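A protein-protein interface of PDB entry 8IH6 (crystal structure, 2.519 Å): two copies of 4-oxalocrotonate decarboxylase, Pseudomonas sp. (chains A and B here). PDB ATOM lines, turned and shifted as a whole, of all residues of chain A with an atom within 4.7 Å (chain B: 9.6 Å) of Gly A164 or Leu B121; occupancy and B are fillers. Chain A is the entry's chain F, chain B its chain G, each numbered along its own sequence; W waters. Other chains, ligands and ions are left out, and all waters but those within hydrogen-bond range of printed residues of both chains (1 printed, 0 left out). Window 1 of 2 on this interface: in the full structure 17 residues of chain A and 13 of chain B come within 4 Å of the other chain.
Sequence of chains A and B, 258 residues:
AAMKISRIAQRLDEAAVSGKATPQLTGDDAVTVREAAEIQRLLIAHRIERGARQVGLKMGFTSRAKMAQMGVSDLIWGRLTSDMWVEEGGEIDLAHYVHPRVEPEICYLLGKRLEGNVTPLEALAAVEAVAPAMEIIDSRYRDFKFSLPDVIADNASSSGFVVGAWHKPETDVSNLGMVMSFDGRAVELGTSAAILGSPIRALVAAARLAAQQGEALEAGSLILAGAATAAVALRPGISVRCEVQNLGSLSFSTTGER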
ATOM      1  N   CYS A 107     -16.540 -13.910  -1.974  1.00  0.00           N
ATOM      2  CA  CYS A 107     -15.807 -13.719  -0.706  1.00  0.00           C
ATOM      3  C   CYS A 107     -15.410 -15.059  -0.111  1.00  0.00           C
ATOM      4  O   CYS A 107     -16.213 -15.947  -0.111  1.00  0.00           O
ATOM      5  CB  CYS A 107     -16.687 -12.966   0.276  1.00  0.00           C
ATOM      6  SG  CYS A 107     -16.140 -13.080   1.989  1.00  0.00           S
ATOM      7  N   LEU A 109     -14.019 -17.188   3.331  1.00  0.00           N
ATOM      8  CA  LEU A 109     -13.862 -17.109   4.795  1.00  0.00           C
ATOM      9  C   LEU A 109     -12.696 -18.015   5.145  1.00  0.00           C
ATOM     10  O   LEU A 109     -12.719 -19.137   4.761  1.00  0.00           O
ATOM     11  CB  LEU A 109     -15.141 -17.581   5.471  1.00  0.00           C
ATOM     12  CG  LEU A 109     -15.024 -17.872   6.955  1.00  0.00           C
ATOM     13  CD1 LEU A 109     -14.464 -16.679   7.676  1.00  0.00           C
ATOM     14  CD2 LEU A 109     -16.360 -18.242   7.535  1.00  0.00           C
ATOM     15  N   ALA A 129     -15.416 -21.629   4.089  1.00  0.00           N
ATOM     16  CA  ALA A 129     -16.600 -21.584   3.241  1.00  0.00           C
ATOM     17  C   ALA A 129     -16.423 -20.474   2.230  1.00  0.00           C
ATOM     18  O   ALA A 129     -15.555 -19.653   2.362  1.00  0.00           O
ATOM     19  CB  ALA A 129     -17.797 -21.334   4.093  1.00  0.00           C
ATOM     20  N   VAL A 130     -17.272 -20.447   1.223  1.00  0.00           N
ATOM     21  CA  VAL A 130     -17.226 -19.388   0.183  1.00  0.00           C
ATOM     22  C   VAL A 130     -18.622 -18.782   0.075  1.00  0.00           C
ATOM     23  O   VAL A 130     -19.549 -19.442   0.402  1.00  0.00           O
ATOM     24  CB  VAL A 130     -16.751 -19.969  -1.150  1.00  0.00           C
ATOM     25  CG1 VAL A 130     -17.732 -20.955  -1.727  1.00  0.00           C
ATOM     26  CG2 VAL A 130     -16.443 -18.889  -2.152  1.00  0.00           C
ATOM     27  N   ALA A 131     -18.743 -17.530  -0.323  1.00  0.00           N
ATOM     28  CA  ALA A 131     -20.083 -16.941  -0.409  1.00  0.00           C
ATOM     29  C   ALA A 131     -20.074 -15.811  -1.405  1.00  0.00           C
ATOM     30  O   ALA A 131     -19.043 -15.310  -1.701  1.00  0.00           O
ATOM     31  CB  ALA A 131     -20.500 -16.420   0.932  1.00  0.00           C
ATOM     32  N   PRO A 132     -21.226 -15.395  -1.925  1.00  0.00           N
ATOM     33  CA  PRO A 132     -21.249 -14.256  -2.794  1.00  0.00           C
ATOM     34  C   PRO A 132     -21.271 -12.984  -1.933  1.00  0.00           C
ATOM     35  O   PRO A 132     -21.586 -13.043  -0.794  1.00  0.00           O
ATOM     36  CB  PRO A 132     -22.525 -14.525  -3.574  1.00  0.00           C
ATOM     37  CG  PRO A 132     -23.408 -15.183  -2.585  1.00  0.00           C
ATOM     38  CD  PRO A 132     -22.499 -16.029  -1.739  1.00  0.00           C
ATOM     39  N   ALA A 133     -20.929 -11.854  -2.528  1.00  0.00           N
ATOM     40  CA  ALA A 133     -20.873 -10.610  -1.744  1.00  0.00           C
ATOM     41  C   ALA A 133     -20.996  -9.390  -2.641  1.00  0.00           C
ATOM     42  O   ALA A 133     -21.030  -9.523  -3.844  1.00  0.00           O
ATOM     43  CB  ALA A 133     -19.566 -10.562  -1.012  1.00  0.00           C
ATOM     44  N   VAL A 162     -20.875  -6.347   2.142  1.00  0.00           N
ATOM     45  CA  VAL A 162     -22.078  -7.124   2.527  1.00  0.00           C
ATOM     46  C   VAL A 162     -21.897  -8.526   1.959  1.00  0.00           C
ATOM     47  O   VAL A 162     -21.500  -8.648   0.828  1.00  0.00           O
ATOM     48  CB  VAL A 162     -23.354  -6.401   2.074  1.00  0.00           C
ATOM     49  CG1 VAL A 162     -23.318  -6.036   0.611  1.00  0.00           C
ATOM     50  CG2 VAL A 162     -24.610  -7.139   2.449  1.00  0.00           C
ATOM     51  N   VAL A 163     -22.168  -9.554   2.753  1.00  0.00           N
ATOM     52  CA  VAL A 163     -21.913 -10.954   2.304  1.00  0.00           C
ATOM     53  C   VAL A 163     -23.201 -11.782   2.306  1.00  0.00           C
ATOM     54  O   VAL A 163     -24.046 -11.547   3.130  1.00  0.00           O
ATOM     55  CB  VAL A 163     -20.803 -11.581   3.172  1.00  0.00           C
ATOM     56  CG1 VAL A 163     -20.298 -12.916   2.678  1.00  0.00           C
ATOM     57  CG2 VAL A 163     -19.627 -10.649   3.302  1.00  0.00           C
ATOM     58  N   GLY A 164     -23.260 -12.776   1.418  1.00  0.00           N
ATOM     59  CA  GLY A 164     -24.355 -13.747   1.281  1.00  0.00           C
ATOM     60  C   GLY A 164     -24.219 -14.952   2.192  1.00  0.00           C
ATOM     61  O   GLY A 164     -23.607 -14.842   3.211  1.00  0.00           O
ATOM     62  N   ALA A 165     -24.771 -16.085   1.780  1.00  0.00           N
ATOM     63  CA  ALA A 165     -24.810 -17.283   2.647  1.00  0.00           C
ATOM     64  C   ALA A 165     -23.573 -18.166   2.522  1.00  0.00           C
ATOM     65  O   ALA A 165     -22.828 -18.016   1.592  1.00  0.00           O
ATOM     66  CB  ALA A 165     -26.057 -18.059   2.370  1.00  0.00           C
ATOM     67  N   TRP A 166     -23.418 -19.049   3.494  1.00  0.00           N
ATOM     68  CA  TRP A 166     -22.329 -20.042   3.609  1.00  0.00           C
ATOM     69  C   TRP A 166     -22.463 -21.088   2.501  1.00  0.00           C
ATOM     70  O   TRP A 166     -23.562 -21.530   2.260  1.00  0.00           O
ATOM     71  CB  TRP A 166     -22.448 -20.676   4.994  1.00  0.00           C
ATOM     72  CG  TRP A 166     -21.369 -21.632   5.378  1.00  0.00           C
ATOM     73  CD1 TRP A 166     -20.382 -21.414   6.277  1.00  0.00           C
ATOM     74  CD2 TRP A 166     -21.177 -22.970   4.910  1.00  0.00           C
ATOM     75  NE1 TRP A 166     -19.591 -22.506   6.399  1.00  0.00           N
ATOM     76  CE2 TRP A 166     -20.052 -23.477   5.569  1.00  0.00           C
ATOM     77  CE3 TRP A 166     -21.831 -23.787   4.000  1.00  0.00           C
ATOM     78  CZ2 TRP A 166     -19.568 -24.758   5.346  1.00  0.00           C
ATOM     79  CZ3 TRP A 166     -21.371 -25.059   3.804  1.00  0.00           C
ATOM     80  CH2 TRP A 166     -20.251 -25.536   4.458  1.00  0.00           C
ATOM     81  N   LEU A 222     -12.013 -12.355   6.241  1.00  0.00           N
ATOM     82  CA  LEU A 222     -12.924 -12.339   5.082  1.00  0.00           C
ATOM     83  C   LEU A 222     -12.088 -11.819   3.927  1.00  0.00           C
ATOM     84  O   LEU A 222     -11.443 -10.813   4.098  1.00  0.00           O
ATOM     85  CB  LEU A 222     -14.093 -11.397   5.344  1.00  0.00           C
ATOM     86  CG  LEU A 222     -15.052 -11.861   6.421  1.00  0.00           C
ATOM     87  CD1 LEU A 222     -16.075 -10.805   6.716  1.00  0.00           C
ATOM     88  CD2 LEU A 222     -15.725 -13.146   6.016  1.00  0.00           C
ATOM     89  N   SER A 249     -28.199 -15.468  -3.328  1.00  0.00           N
ATOM     90  CA  SER A 249     -28.186 -14.003  -3.502  1.00  0.00           C
ATOM     91  C   SER A 249     -28.028 -13.271  -2.173  1.00  0.00           C
ATOM     92  O   SER A 249     -28.121 -13.868  -1.125  1.00  0.00           O
ATOM     93  CB  SER A 249     -29.432 -13.565  -4.186  1.00  0.00           C
ATOM     94  OG  SER A 249     -30.550 -14.011  -3.466  1.00  0.00           O
ATOM     95  N   LEU A 250     -27.769 -11.980  -2.271  1.00  0.00           N
ATOM     96  CA  LEU A 250     -27.658 -11.110  -1.082  1.00  0.00           C
ATOM     97  C   LEU A 250     -28.219  -9.745  -1.443  1.00  0.00           C
ATOM     98  O   LEU A 250     -28.251  -9.424  -2.610  1.00  0.00           O
ATOM     99  CB  LEU A 250     -26.209 -11.033  -0.609  1.00  0.00           C
ATOM    100  CG  LEU A 250     -25.219 -10.398  -1.566  1.00  0.00           C
ATOM    101  CD1 LEU A 250     -24.221  -9.578  -0.796  1.00  0.00           C
ATOM    102  CD2 LEU A 250     -24.516 -11.460  -2.365  1.00  0.00           C
ATOM    103  N   LYS B 112     -20.195 -23.553  17.537  1.00  0.00           N
ATOM    104  CA  LYS B 112     -19.162 -22.675  18.109  1.00  0.00           C
ATOM    105  C   LYS B 112     -19.799 -21.364  18.551  1.00  0.00           C
ATOM    106  O   LYS B 112     -20.914 -21.115  18.205  1.00  0.00           O
ATOM    107  CB  LYS B 112     -18.071 -22.343  17.093  1.00  0.00           C
ATOM    108  CG  LYS B 112     -17.510 -23.475  16.256  1.00  0.00           C
ATOM    109  CD  LYS B 112     -16.638 -22.915  15.165  1.00  0.00           C
ATOM    110  CE  LYS B 112     -15.753 -23.910  14.456  1.00  0.00           C
ATOM    111  NZ  LYS B 112     -15.504 -23.494  13.055  1.00  0.00           N
ATOM    112  N   LEU B 114     -20.745 -17.581  18.563  1.00  0.00           N
ATOM    113  CA  LEU B 114     -21.019 -16.555  17.537  1.00  0.00           C
ATOM    114  C   LEU B 114     -21.181 -15.232  18.275  1.00  0.00           C
ATOM    115  O   LEU B 114     -21.924 -15.211  19.233  1.00  0.00           O
ATOM    116  CB  LEU B 114     -22.306 -16.933  16.822  1.00  0.00           C
ATOM    117  CG  LEU B 114     -22.440 -16.328  15.442  1.00  0.00           C
ATOM    118  CD1 LEU B 114     -21.255 -16.710  14.590  1.00  0.00           C
ATOM    119  CD2 LEU B 114     -23.741 -16.746  14.806  1.00  0.00           C
ATOM    120  N   VAL B 118     -22.028 -10.138  12.487  1.00  0.00           N
ATOM    121  CA  VAL B 118     -21.594 -11.297  11.663  1.00  0.00           C
ATOM    122  C   VAL B 118     -22.305 -11.333  10.313  1.00  0.00           C
ATOM    123  O   VAL B 118     -23.441 -10.971  10.255  1.00  0.00           O
ATOM    124  CB  VAL B 118     -21.950 -12.575  12.424  1.00  0.00           C
ATOM    125  CG1 VAL B 118     -21.543 -12.474  13.873  1.00  0.00           C
ATOM    126  CG2 VAL B 118     -23.436 -12.833  12.330  1.00  0.00           C
ATOM    127  N   THR B 119     -21.624 -11.811   9.285  1.00  0.00           N
ATOM    128  CA  THR B 119     -22.276 -11.999   7.974  1.00  0.00           C
ATOM    129  C   THR B 119     -22.998 -13.351   7.972  1.00  0.00           C
ATOM    130  O   THR B 119     -22.743 -14.154   8.844  1.00  0.00           O
ATOM    131  CB  THR B 119     -21.266 -11.967   6.830  1.00  0.00           C
ATOM    132  OG1 THR B 119     -20.415 -13.068   7.064  1.00  0.00           O
ATOM    133  CG2 THR B 119     -20.437 -10.716   6.754  1.00  0.00           C
ATOM    134  N   PRO B 120     -23.902 -13.632   7.016  1.00  0.00           N
ATOM    135  CA  PRO B 120     -24.581 -14.911   6.944  1.00  0.00           C
ATOM    136  C   PRO B 120     -23.562 -16.042   6.821  1.00  0.00           C
ATOM    137  O   PRO B 120     -23.743 -17.022   7.430  1.00  0.00           O
ATOM    138  CB  PRO B 120     -25.376 -14.794   5.652  1.00  0.00           C
ATOM    139  CG  PRO B 120     -25.648 -13.349   5.554  1.00  0.00           C
ATOM    140  CD  PRO B 120     -24.349 -12.730   5.985  1.00  0.00           C
ATOM    141  N   LEU B 121     -22.550 -15.849   5.988  1.00  0.00           N
ATOM    142  CA  LEU B 121     -21.442 -16.803   5.813  1.00  0.00           C
ATOM    143  C   LEU B 121     -20.817 -17.123   7.167  1.00  0.00           C
ATOM    144  O   LEU B 121     -20.715 -18.277   7.466  1.00  0.00           O
ATOM    145  CB  LEU B 121     -20.444 -16.146   4.871  1.00  0.00           C
ATOM    146  CG  LEU B 121     -19.036 -16.702   4.862  1.00  0.00           C
ATOM    147  CD1 LEU B 121     -19.035 -18.158   4.486  1.00  0.00           C
ATOM    148  CD2 LEU B 121     -18.207 -15.929   3.873  1.00  0.00           C
ATOM    149  N   GLU B 122     -20.456 -16.132   7.976  1.00  0.00           N
ATOM    150  CA  GLU B 122     -19.810 -16.480   9.262  1.00  0.00           C
ATOM    151  C   GLU B 122     -20.829 -17.052  10.235  1.00  0.00           C
ATOM    152  O   GLU B 122     -20.430 -17.801  11.096  1.00  0.00           O
ATOM    153  CB  GLU B 122     -19.125 -15.279   9.898  1.00  0.00           C
ATOM    154  CG  GLU B 122     -18.268 -14.482   8.955  1.00  0.00           C
ATOM    155  CD  GLU B 122     -17.812 -13.172   9.544  1.00  0.00           C
ATOM    156  OE1 GLU B 122     -18.405 -12.165   9.224  1.00  0.00           O
ATOM    157  OE2 GLU B 122     -16.872 -13.190  10.324  1.00  0.00           O
ATOM    158  N   ALA B 123     -22.091 -16.684  10.103  1.00  0.00           N
ATOM    159  CA  ALA B 123     -23.105 -17.192  11.041  1.00  0.00           C
ATOM    160  C   ALA B 123     -23.224 -18.703  10.898  1.00  0.00           C
ATOM    161  O   ALA B 123     -23.279 -19.364  11.895  1.00  0.00           O
ATOM    162  CB  ALA B 123     -24.420 -16.505  10.809  1.00  0.00           C
ATOM    163  N   LEU B 124     -23.283 -19.196   9.664  1.00  0.00           N
ATOM    164  CA  LEU B 124     -23.472 -20.645   9.443  1.00  0.00           C
ATOM    165  C   LEU B 124     -22.207 -21.416   9.735  1.00  0.00           C
ATOM    166  O   LEU B 124     -22.300 -22.586   9.935  1.00  0.00           O
ATOM    167  CB  LEU B 124     -23.977 -20.955   8.043  1.00  0.00           C
ATOM    168  CG  LEU B 124     -24.673 -22.300   7.977  1.00  0.00           C
ATOM    169  CD1 LEU B 124     -25.967 -22.251   8.741  1.00  0.00           C
ATOM    170  CD2 LEU B 124     -24.889 -22.719   6.553  1.00  0.00           C
ATOM    171  N   ALA B 125     -21.070 -20.754   9.791  1.00  0.00           N
ATOM    172  CA  ALA B 125     -19.833 -21.492  10.087  1.00  0.00           C
ATOM    173  C   ALA B 125     -19.836 -21.933  11.547  1.00  0.00           C
ATOM    174  O   ALA B 125     -19.103 -22.841  11.884  1.00  0.00           O
ATOM    175  CB  ALA B 125     -18.658 -20.640   9.760  1.00  0.00           C
ATOM    176  N   ALA B 126     -20.684 -21.330  12.363  1.00  0.00           N
ATOM    177  CA  ALA B 126     -20.752 -21.681  13.789  1.00  0.00           C
ATOM    178  C   ALA B 126     -21.974 -22.548  14.048  1.00  0.00           C
ATOM    179  O   ALA B 126     -22.238 -22.863  15.180  1.00  0.00           O
ATOM    180  CB  ALA B 126     -20.818 -20.427  14.594  1.00  0.00           C
ATOM    181  N   VAL B 127     -22.644 -23.016  13.009  1.00  0.00           N
ATOM    182  CA  VAL B 127     -23.890 -23.797  13.243  1.00  0.00           C
ATOM    183  C   VAL B 127     -23.638 -25.299  13.173  1.00  0.00           C
ATOM    184  O   VAL B 127     -23.053 -25.725  12.237  1.00  0.00           O
ATOM    185  CB  VAL B 127     -24.999 -23.356  12.280  1.00  0.00           C
ATOM    186  CG1 VAL B 127     -26.177 -24.293  12.330  1.00  0.00           C
ATOM    187  CG2 VAL B 127     -25.433 -21.940  12.564  1.00  0.00           C
ATOM    188  N   PRO B 169     -26.311 -28.631   8.748  1.00  0.00           N
ATOM    189  CA  PRO B 169     -26.265 -27.174   8.738  1.00  0.00           C
ATOM    190  C   PRO B 169     -26.290 -26.477   7.372  1.00  0.00           C
ATOM    191  O   PRO B 169     -26.736 -25.409   7.288  1.00  0.00           O
ATOM    192  CB  PRO B 169     -24.946 -26.879   9.436  1.00  0.00           C
ATOM    193  CG  PRO B 169     -24.165 -28.112   9.232  1.00  0.00           C
ATOM    194  CD  PRO B 169     -25.179 -29.196   9.443  1.00  0.00           C
ATOM    195  N   SER B 198     -35.248 -14.733   5.126  1.00  0.00           N
ATOM    196  CA  SER B 198     -34.211 -15.788   5.156  1.00  0.00           C
ATOM    197  C   SER B 198     -33.914 -16.049   6.614  1.00  0.00           C
ATOM    198  O   SER B 198     -33.401 -15.172   7.234  1.00  0.00           O
ATOM    199  CB  SER B 198     -32.952 -15.320   4.519  1.00  0.00           C
ATOM    200  OG  SER B 198     -32.375 -16.341   3.745  1.00  0.00           O
ATOM    201  N   ILE B 200     -31.413 -17.312   8.173  1.00  0.00           N
ATOM    202  CA  ILE B 200     -30.015 -16.978   8.530  1.00  0.00           C
ATOM    203  C   ILE B 200     -29.950 -15.529   9.005  1.00  0.00           C
ATOM    204  O   ILE B 200     -29.138 -15.272   9.858  1.00  0.00           O
ATOM    205  CB  ILE B 200     -29.064 -17.270   7.352  1.00  0.00           C
ATOM    206  CG1 ILE B 200     -27.625 -17.444   7.817  1.00  0.00           C
ATOM    207  CG2 ILE B 200     -29.165 -16.234   6.262  1.00  0.00           C
ATOM    208  CD1 ILE B 200     -27.453 -18.475   8.869  1.00  0.00           C
ATOM    209  N   ARG B 201     -30.849 -14.664   8.536  1.00  0.00           N
ATOM    210  CA  ARG B 201     -30.780 -13.235   8.900  1.00  0.00           C
ATOM    211  C   ARG B 201     -31.088 -13.075  10.381  1.00  0.00           C
ATOM    212  O   ARG B 201     -30.564 -12.167  10.980  1.00  0.00           O
ATOM    213  CB  ARG B 201     -31.796 -12.477   8.056  1.00  0.00           C
ATOM    214  CG  ARG B 201     -31.305 -12.122   6.667  1.00  0.00           C
ATOM    215  CD  ARG B 201     -32.432 -11.915   5.705  1.00  0.00           C
ATOM    216  NE  ARG B 201     -31.847 -11.388   4.503  1.00  0.00           N
ATOM    217  CZ  ARG B 201     -32.529 -10.986   3.463  1.00  0.00           C
ATOM    218  NH1 ARG B 201     -33.838 -11.062   3.480  1.00  0.00           N
ATOM    219  NH2 ARG B 201     -31.908 -10.513   2.411  1.00  0.00           N
ATOM    220  N   LEU B 203     -30.376 -15.269  12.780  1.00  0.00           N
ATOM    221  CA  LEU B 203     -29.217 -15.710  13.577  1.00  0.00           C
ATOM    222  C   LEU B 203     -28.243 -14.543  13.645  1.00  0.00           C
ATOM    223  O   LEU B 203     -27.732 -14.295  14.711  1.00  0.00           O
ATOM    224  CB  LEU B 203     -28.605 -16.932  12.903  1.00  0.00           C
ATOM    225  CG  LEU B 203     -27.517 -17.631  13.701  1.00  0.00           C
ATOM    226  CD1 LEU B 203     -28.004 -17.969  15.089  1.00  0.00           C
ATOM    227  CD2 LEU B 203     -27.042 -18.863  12.981  1.00  0.00           C
ATOM    228  N   VAL B 204     -28.052 -13.847  12.533  1.00  0.00           N
ATOM    229  CA  VAL B 204     -27.183 -12.645  12.474  1.00  0.00           C
ATOM    230  C   VAL B 204     -27.712 -11.647  13.497  1.00  0.00           C
ATOM    231  O   VAL B 204     -26.949 -11.157  14.293  1.00  0.00           O
ATOM    232  CB  VAL B 204     -27.224 -12.035  11.072  1.00  0.00           C
ATOM    233  CG1 VAL B 204     -26.450 -10.738  10.983  1.00  0.00           C
ATOM    234  CG2 VAL B 204     -26.730 -13.007  10.041  1.00  0.00           C
HETATM  235  O   HOH W   1     -25.163 -18.617   5.608  1.00  0.00           O
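The backbone carbonyl oxygen of Gly A164 is in hydrogen-bond range of the backbone NH of Leu B121.
The backbone NH (N) of Cys A107 lies within hydrogen-bond range of the backbone carbonyl oxygen (O) of Ala A131 (2.9 Å). The backbone carbonyl oxygen (O) of Ala A129 is in hydrogen-bond range of the backbone NH (N) of Leu A109, at 3.1 Å. O of Pro A132 sits at hydrogen-bond distance from N of Gly A164 (2.8 Å). OG1 of Thr B119 lies within hydrogen-bond range of OE1 of Glu B122, 3.1 Å away.
Among the printed residues, pairs that only touch across the chains: Gly A164 with Pro B120 (3.0 Å), Val A163 with Pro B120 (3.1 Å), Trp A166 with Leu B121 (3.4 Å), Trp A166 with Leu B124 (3.4 Å), Ala A129 with Leu B121 (3.4 Å), Val A163 with Thr B119 (3.5 Å), Trp A166 with Ala B125 (3.6 Å), Leu A222 with Glu B122 (3.7 Å), Ala A131 with Leu B121 (3.8 Å), Leu A109 with Leu B121 (3.8 Å), Val A163 with Leu B121 (3.9 Å), Ala A165 with Pro B120 (3.9 Å), Cys A107 with Leu B121 (3.99 Å) and Leu A109 with Ala B125 (3.998 Å).
Gly A164 touches just these residues of chain B: Pro B120 and Leu B121. Printed residues of chain A within 4 Å of Leu B121: Cys A107, Leu A109, Ala A129, Ala A131, Val A163, Gly A164 and Trp A166. Ala A129 touches one residue of chain B. No residue of chain B comes within 4 Å of Pro A132. Of the printed residues of chain B, Trp A166 touches Leu B121 (3.4 Å), Leu B124 (3.4 Å) and Ala B125 (3.6 Å). Of the printed residues of chain A, Thr B119 touches Val A163. Leu A250 touches none of the printed residues of chain B. The nearest printed residue of chain A that does not touch Leu B121 is Ala A165 (4.2 Å). The nearest printed residue of chain A that does not touch Leu B124 is Ala A165 (6.2 Å).
Of the 18 printed residues of chain B, 6 touch a printed residue of chain A. Hydrophobic or aromatic side chains of chain B that line the printed part of chain A: Pro B120, Leu B121, Leu B124 and Ala B125. Among the printed residues, 15 pairs touch across the chains.
No position is printed for both chains. Of the 15 pairs that touch across the chains among the printed residues, none has its exchanged pair printed and touching as well.
Water W1 bridges the backbone NH (N) of Trp A166 (2.8 Å) and the backbone carbonyl oxygen (O) of Pro B120 (2.8 Å).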
